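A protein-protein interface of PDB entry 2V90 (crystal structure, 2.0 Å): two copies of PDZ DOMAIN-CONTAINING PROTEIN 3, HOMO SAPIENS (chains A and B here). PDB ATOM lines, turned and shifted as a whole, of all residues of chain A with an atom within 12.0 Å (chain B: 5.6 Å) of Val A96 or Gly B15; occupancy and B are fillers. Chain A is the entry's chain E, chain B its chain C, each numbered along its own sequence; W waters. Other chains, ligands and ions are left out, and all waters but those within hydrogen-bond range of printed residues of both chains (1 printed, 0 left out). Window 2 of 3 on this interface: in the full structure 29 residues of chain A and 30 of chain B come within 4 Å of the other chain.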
ATOM      1  N   ASP A  91      -5.470 -11.061  29.281  1.00  0.00           N
ATOM      2  CA  ASP A  91      -4.115 -11.226  28.749  1.00  0.00           C
ATOM      3  C   ASP A  91      -3.816 -10.426  27.464  1.00  0.00           C
ATOM      4  O   ASP A  91      -2.762 -10.605  26.859  1.00  0.00           O
ATOM      5  CB  ASP A  91      -3.873 -12.710  28.470  1.00  0.00           C
ATOM      6  CG  ASP A  91      -4.902 -13.297  27.504  1.00  0.00           C
ATOM      7  OD1 ASP A  91      -6.105 -12.952  27.623  1.00  0.00           O
ATOM      8  OD2 ASP A  91      -4.505 -14.100  26.635  1.00  0.00           O
ATOM      9  N   ARG A  92      -4.724  -9.558  27.030  1.00  0.00           N
ATOM     10  CA  ARG A  92      -4.473  -8.778  25.826  1.00  0.00           C
ATOM     11  C   ARG A  92      -4.255  -7.318  26.182  1.00  0.00           C
ATOM     12  O   ARG A  92      -4.739  -6.422  25.514  1.00  0.00           O
ATOM     13  CB  ARG A  92      -5.560  -9.010  24.764  1.00  0.00           C
ATOM     14  CG  ARG A  92      -5.785 -10.487  24.478  1.00  0.00           C
ATOM     15  CD  ARG A  92      -5.922 -10.790  23.043  1.00  0.00           C
ATOM     16  NE  ARG A  92      -6.215 -12.207  22.799  1.00  0.00           N
ATOM     17  CZ  ARG A  92      -6.988 -12.676  21.815  1.00  0.00           C
ATOM     18  NH1 ARG A  92      -7.589 -11.860  20.966  1.00  0.00           N
ATOM     19  NH2 ARG A  92      -7.174 -13.982  21.677  1.00  0.00           N
ATOM     20  N   GLU A  93      -3.491  -7.118  27.262  1.00  0.00           N
ATOM     21  CA  GLU A  93      -2.951  -5.828  27.682  1.00  0.00           C
ATOM     22  C   GLU A  93      -1.502  -6.068  28.115  1.00  0.00           C
ATOM     23  O   GLU A  93      -1.212  -7.035  28.803  1.00  0.00           O
ATOM     24  CB  GLU A  93      -3.755  -5.227  28.858  1.00  0.00           C
ATOM     25  CG  GLU A  93      -3.929  -6.178  30.067  1.00  0.00           C
ATOM     26  CD  GLU A  93      -4.000  -5.447  31.416  1.00  0.00           C
ATOM     27  OE1 GLU A  93      -3.436  -5.972  32.415  1.00  0.00           O
ATOM     28  OE2 GLU A  93      -4.589  -4.344  31.473  1.00  0.00           O
ATOM     29  N   THR A  94      -0.594  -5.205  27.694  1.00  0.00           N
ATOM     30  CA  THR A  94       0.799  -5.337  28.048  1.00  0.00           C
ATOM     31  C   THR A  94       1.447  -3.987  28.264  1.00  0.00           C
ATOM     32  O   THR A  94       1.289  -3.074  27.450  1.00  0.00           O
ATOM     33  CB  THR A  94       1.585  -6.082  26.936  1.00  0.00           C
ATOM     34  OG1 THR A  94       0.937  -7.335  26.624  1.00  0.00           O
ATOM     35  CG2 THR A  94       3.019  -6.303  27.355  1.00  0.00           C
ATOM     36  N   SER A  95       2.190  -3.876  29.363  1.00  0.00           N
ATOM     37  CA  SER A  95       2.971  -2.695  29.649  1.00  0.00           C
ATOM     38  C   SER A  95       4.345  -2.863  29.014  1.00  0.00           C
ATOM     39  O   SER A  95       5.045  -3.851  29.271  1.00  0.00           O
ATOM     40  CB  SER A  95       3.070  -2.461  31.170  1.00  0.00           C
ATOM     41  OG  SER A  95       3.951  -1.385  31.475  1.00  0.00           O
ATOM     42  N   VAL A  96       4.721  -1.923  28.148  1.00  0.00           N
ATOM     43  CA  VAL A  96       6.011  -1.985  27.445  1.00  0.00           C
ATOM     44  C   VAL A  96       6.856  -0.752  27.798  1.00  0.00           C
ATOM     45  O   VAL A  96       6.326   0.264  28.226  1.00  0.00           O
ATOM     46  CB  VAL A  96       5.824  -2.103  25.890  1.00  0.00           C
ATOM     47  CG1 VAL A  96       5.063  -3.380  25.510  1.00  0.00           C
ATOM     48  CG2 VAL A  96       5.094  -0.895  25.336  1.00  0.00           C
ATOM     49  OXT VAL A  96       8.078  -0.710  27.655  1.00  0.00           O
ATOM     50  N   GLU B  10      13.444   5.998  22.692  1.00  0.00           N
ATOM     51  CA  GLU B  10      14.577   5.349  23.313  1.00  0.00           C
ATOM     52  C   GLU B  10      14.127   4.741  24.650  1.00  0.00           C
ATOM     53  O   GLU B  10      13.552   5.415  25.496  1.00  0.00           O
ATOM     54  CB  GLU B  10      15.709   6.358  23.532  1.00  0.00           C
ATOM     55  CG  GLU B  10      17.076   5.726  23.763  1.00  0.00           C
ATOM     56  N   LYS B  11      14.399   3.459  24.828  1.00  0.00           N
ATOM     57  CA  LYS B  11      13.945   2.699  25.979  1.00  0.00           C
ATOM     58  C   LYS B  11      14.753   3.070  27.202  1.00  0.00           C
ATOM     59  O   LYS B  11      15.946   3.371  27.113  1.00  0.00           O
ATOM     60  CB  LYS B  11      14.143   1.217  25.661  1.00  0.00           C
ATOM     61  CG  LYS B  11      13.478   0.183  26.534  1.00  0.00           C
ATOM     62  CD  LYS B  11      13.375  -1.117  25.710  1.00  0.00           C
ATOM     63  CE  LYS B  11      13.272  -2.343  26.529  1.00  0.00           C
ATOM     64  NZ  LYS B  11      13.487  -3.531  25.667  1.00  0.00           N
ATOM     65  N   GLY B  12      14.107   3.029  28.359  1.00  0.00           N
ATOM     66  CA  GLY B  12      14.801   3.287  29.619  1.00  0.00           C
ATOM     67  C   GLY B  12      14.797   2.044  30.482  1.00  0.00           C
ATOM     68  O   GLY B  12      14.435   0.953  30.026  1.00  0.00           O
ATOM     69  N   PRO B  13      15.181   2.196  31.745  1.00  0.00           N
ATOM     70  CA  PRO B  13      15.304   1.014  32.601  1.00  0.00           C
ATOM     71  C   PRO B  13      13.929   0.387  32.857  1.00  0.00           C
ATOM     72  O   PRO B  13      13.805  -0.832  33.013  1.00  0.00           O
ATOM     73  CB  PRO B  13      15.936   1.564  33.889  1.00  0.00           C
ATOM     74  CG  PRO B  13      16.348   2.956  33.587  1.00  0.00           C
ATOM     75  CD  PRO B  13      15.498   3.437  32.461  1.00  0.00           C
ATOM     76  N   GLN B  14      12.897   1.219  32.867  1.00  0.00           N
ATOM     77  CA  GLN B  14      11.546   0.718  32.992  1.00  0.00           C
ATOM     78  C   GLN B  14      10.771   0.817  31.681  1.00  0.00           C
ATOM     79  O   GLN B  14       9.572   1.025  31.694  1.00  0.00           O
ATOM     80  CB  GLN B  14      10.832   1.447  34.129  1.00  0.00           C
ATOM     81  CG  GLN B  14      11.414   1.129  35.506  1.00  0.00           C
ATOM     82  CD  GLN B  14      11.285  -0.355  35.900  1.00  0.00           C
ATOM     83  OE1 GLN B  14      10.182  -0.859  36.120  1.00  0.00           O
ATOM     84  NE2 GLN B  14      12.423  -1.042  36.014  1.00  0.00           N
ATOM     85  N   GLY B  15      11.451   0.635  30.548  1.00  0.00           N
ATOM     86  CA  GLY B  15      10.756   0.443  29.275  1.00  0.00           C
ATOM     87  C   GLY B  15      10.415   1.743  28.575  1.00  0.00           C
ATOM     88  O   GLY B  15      11.021   2.769  28.844  1.00  0.00           O
ATOM     89  N   PHE B  16       9.449   1.691  27.671  1.00  0.00           N
ATOM     90  CA  PHE B  16       9.020   2.858  26.850  1.00  0.00           C
ATOM     91  C   PHE B  16       8.003   3.795  27.521  1.00  0.00           C
ATOM     92  O   PHE B  16       7.939   4.995  27.216  1.00  0.00           O
ATOM     93  CB  PHE B  16       8.492   2.350  25.495  1.00  0.00           C
ATOM     94  CG  PHE B  16       9.565   1.702  24.645  1.00  0.00           C
ATOM     95  CD1 PHE B  16      10.618   2.457  24.169  1.00  0.00           C
ATOM     96  CD2 PHE B  16       9.521   0.351  24.318  1.00  0.00           C
ATOM     97  CE1 PHE B  16      11.621   1.887  23.382  1.00  0.00           C
ATOM     98  CE2 PHE B  16      10.524  -0.213  23.540  1.00  0.00           C
ATOM     99  CZ  PHE B  16      11.568   0.554  23.076  1.00  0.00           C
ATOM    100  N   GLY B  17       7.240   3.258  28.458  1.00  0.00           N
ATOM    101  CA  GLY B  17       6.249   4.014  29.174  1.00  0.00           C
ATOM    102  C   GLY B  17       4.846   4.054  28.580  1.00  0.00           C
ATOM    103  O   GLY B  17       4.218   5.097  28.580  1.00  0.00           O
ATOM    104  N   PHE B  18       4.354   2.923  28.083  1.00  0.00           N
ATOM    105  CA  PHE B  18       2.919   2.801  27.734  1.00  0.00           C
ATOM    106  C   PHE B  18       2.306   1.426  27.996  1.00  0.00           C
ATOM    107  O   PHE B  18       2.996   0.396  28.073  1.00  0.00           O
ATOM    108  CB  PHE B  18       2.633   3.284  26.292  1.00  0.00           C
ATOM    109  CG  PHE B  18       3.315   2.486  25.204  1.00  0.00           C
ATOM    110  CD1 PHE B  18       2.651   1.454  24.561  1.00  0.00           C
ATOM    111  CD2 PHE B  18       4.580   2.821  24.771  1.00  0.00           C
ATOM    112  CE1 PHE B  18       3.275   0.743  23.533  1.00  0.00           C
ATOM    113  CE2 PHE B  18       5.223   2.113  23.757  1.00  0.00           C
ATOM    114  CZ  PHE B  18       4.576   1.087  23.135  1.00  0.00           C
ATOM    115  N   LEU B  19       0.982   1.441  28.175  1.00  0.00           N
ATOM    116  CA  LEU B  19       0.127   0.249  28.290  1.00  0.00           C
ATOM    117  C   LEU B  19      -0.568   0.052  26.951  1.00  0.00           C
ATOM    118  O   LEU B  19      -1.290   0.950  26.518  1.00  0.00           O
ATOM    119  CB  LEU B  19      -0.962   0.505  29.345  1.00  0.00           C
ATOM    120  CG  LEU B  19      -1.953  -0.628  29.626  1.00  0.00           C
ATOM    121  CD1 LEU B  19      -1.177  -1.795  30.215  1.00  0.00           C
ATOM    122  CD2 LEU B  19      -2.988  -0.147  30.613  1.00  0.00           C
ATOM    123  N   LEU B  20      -0.307  -1.051  26.266  1.00  0.00           N
ATOM    124  CA  LEU B  20      -1.046  -1.392  25.028  1.00  0.00           C
ATOM    125  C   LEU B  20      -2.174  -2.351  25.378  1.00  0.00           C
ATOM    126  O   LEU B  20      -1.956  -3.312  26.104  1.00  0.00           O
ATOM    127  CB  LEU B  20      -0.112  -2.033  24.019  1.00  0.00           C
ATOM    128  CG  LEU B  20      -0.514  -2.159  22.566  1.00  0.00           C
ATOM    129  CD1 LEU B  20      -0.678  -0.762  21.904  1.00  0.00           C
ATOM    130  CD2 LEU B  20       0.534  -3.015  21.856  1.00  0.00           C
ATOM    131  N   ASP B  38       2.644   6.560  30.420  1.00  0.00           N
ATOM    132  CA  ASP B  38       3.198   6.851  31.756  1.00  0.00           C
ATOM    133  C   ASP B  38       3.893   8.198  31.831  1.00  0.00           C
ATOM    134  O   ASP B  38       4.690   8.539  30.971  1.00  0.00           O
ATOM    135  CB  ASP B  38       4.134   5.726  32.216  1.00  0.00           C
ATOM    136  CG  ASP B  38       3.458   4.337  32.105  1.00  0.00           C
ATOM    137  OD1 ASP B  38       2.349   4.178  32.665  1.00  0.00           O
ATOM    138  OD2 ASP B  38       3.996   3.428  31.431  1.00  0.00           O
ATOM    139  N   LEU B  41       8.183   9.241  31.258  1.00  0.00           N
ATOM    140  CA  LEU B  41       8.826   8.120  30.572  1.00  0.00           C
ATOM    141  C   LEU B  41       8.806   8.391  29.070  1.00  0.00           C
ATOM    142  O   LEU B  41       8.094   9.313  28.639  1.00  0.00           O
ATOM    143  CB  LEU B  41       8.143   6.803  30.935  1.00  0.00           C
ATOM    144  CG  LEU B  41       8.336   6.219  32.352  1.00  0.00           C
ATOM    145  CD1 LEU B  41       7.855   4.788  32.413  1.00  0.00           C
ATOM    146  CD2 LEU B  41       9.790   6.281  32.802  1.00  0.00           C
ATOM    147  N   PRO B  42       9.640   7.659  28.285  1.00  0.00           N
ATOM    148  CA  PRO B  42       9.890   7.952  26.867  1.00  0.00           C
ATOM    149  C   PRO B  42       8.687   8.243  25.984  1.00  0.00           C
ATOM    150  O   PRO B  42       8.702   9.233  25.269  1.00  0.00           O
ATOM    151  CB  PRO B  42      10.680   6.730  26.397  1.00  0.00           C
ATOM    152  CG  PRO B  42      11.502   6.413  27.611  1.00  0.00           C
ATOM    153  CD  PRO B  42      10.494   6.531  28.726  1.00  0.00           C
ATOM    154  N   VAL B  71       3.201  -6.922  20.309  1.00  0.00           N
ATOM    155  CA  VAL B  71       4.201  -6.774  21.374  1.00  0.00           C
ATOM    156  C   VAL B  71       5.541  -7.374  20.934  1.00  0.00           C
ATOM    157  O   VAL B  71       6.609  -6.789  21.168  1.00  0.00           O
ATOM    158  CB  VAL B  71       3.746  -7.481  22.712  1.00  0.00           C
ATOM    159  CG1 VAL B  71       4.878  -7.378  23.815  1.00  0.00           C
ATOM    160  CG2 VAL B  71       2.459  -6.875  23.193  1.00  0.00           C
ATOM    161  N   ILE B  74       7.416  -4.967  18.754  1.00  0.00           N
ATOM    162  CA  ILE B  74       8.007  -3.885  19.578  1.00  0.00           C
ATOM    163  C   ILE B  74       9.216  -4.417  20.366  1.00  0.00           C
ATOM    164  O   ILE B  74      10.266  -3.780  20.414  1.00  0.00           O
ATOM    165  CB  ILE B  74       6.952  -3.296  20.569  1.00  0.00           C
ATOM    166  CG1 ILE B  74       5.797  -2.610  19.811  1.00  0.00           C
ATOM    167  CG2 ILE B  74       7.611  -2.389  21.629  1.00  0.00           C
ATOM    168  CD1 ILE B  74       4.583  -2.380  20.700  1.00  0.00           C
HETATM  169  O   HOH W   1       2.157   1.034  31.757  1.00  0.00           O
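N of Val A96 lies within hydrogen-bond range of O of Phe B18, 2.9 Å away. The backbone carbonyl oxygen (O) of Leu B20 lies within hydrogen-bond range of the backbone NH (N) of Thr A94 (2.8 Å). N of Gly B17 sits at hydrogen-bond distance from O of Val A96, 3.1 Å away. The backbone NH (N) of Phe B16 lies within hydrogen-bond range of the chain-end carboxylate (OXT) of Val A96.
The side-chain carboxylate (OD2) of Asp B38 sits at hydrogen-bond distance from the backbone NH (N) of Phe B18 (3.4 Å). N of Asp B38 lies within hydrogen-bond range of O of Gly B17, 2.8 Å away.
O of Leu B20 touches CA of Glu A93 (3.1 Å). Thr A94 touches Phe B18 (O to O, 3.9 Å). CA of Leu B19 touches O of Thr A94 (3.6 Å). Val B71 touches Thr A94. Ser A95 touches Phe B18. Val A96 touches Gly B15 (OXT to CA, 3.3 Å).
Val A96 touches four residues of chain B. Of chain A, only Val A96 comes within 4 Å of Gly B15. No residue of chain A comes within 4 Å of Lys B11. No residue of chain A comes within 4 Å of Gly B12. No residue of chain A comes within 4 Å of Gln B14. Of chain A, only Val A96 comes within 4 Å of Phe B16. Of the printed residues of chain A, Gly B17 touches Val A96. Phe B18 touches three residues of chain A. No residue of chain A comes within 4 Å of Leu B41. No residue of chain A comes within 4 Å of Pro B42. Printed residues of chain B within 4 Å of Glu A93: Leu B20. Of the printed residues of chain B, Thr A94 touches Phe B18, Leu B19, Leu B20 and Val B71. Printed residues of chain B within 4 Å of Ser A95: Phe B18 (3.5 Å). Of the printed residues of chain A, Leu B19 touches Thr A94 (3.6 Å).
Printed residues of chain A that touch a printed residue of chain B: Glu A93, Thr A94, Ser A95 and Val A96. Hydrophobic or aromatic side chains of chain A that line the printed part of chain B: Val A96. Among the printed residues, no Asp or Glu carboxylate lies within 4 Å of a Lys or Arg side-chain nitrogen of the other chain.
No position is printed for both chains. Of the 10 pairs that touch across the chains among the printed residues, none has its exchanged pair printed and touching as well.
Water W1 lies within hydrogen-bond range of OG of Ser A95 (3.0 Å) and OD2 of Asp B38 (3.0 Å).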
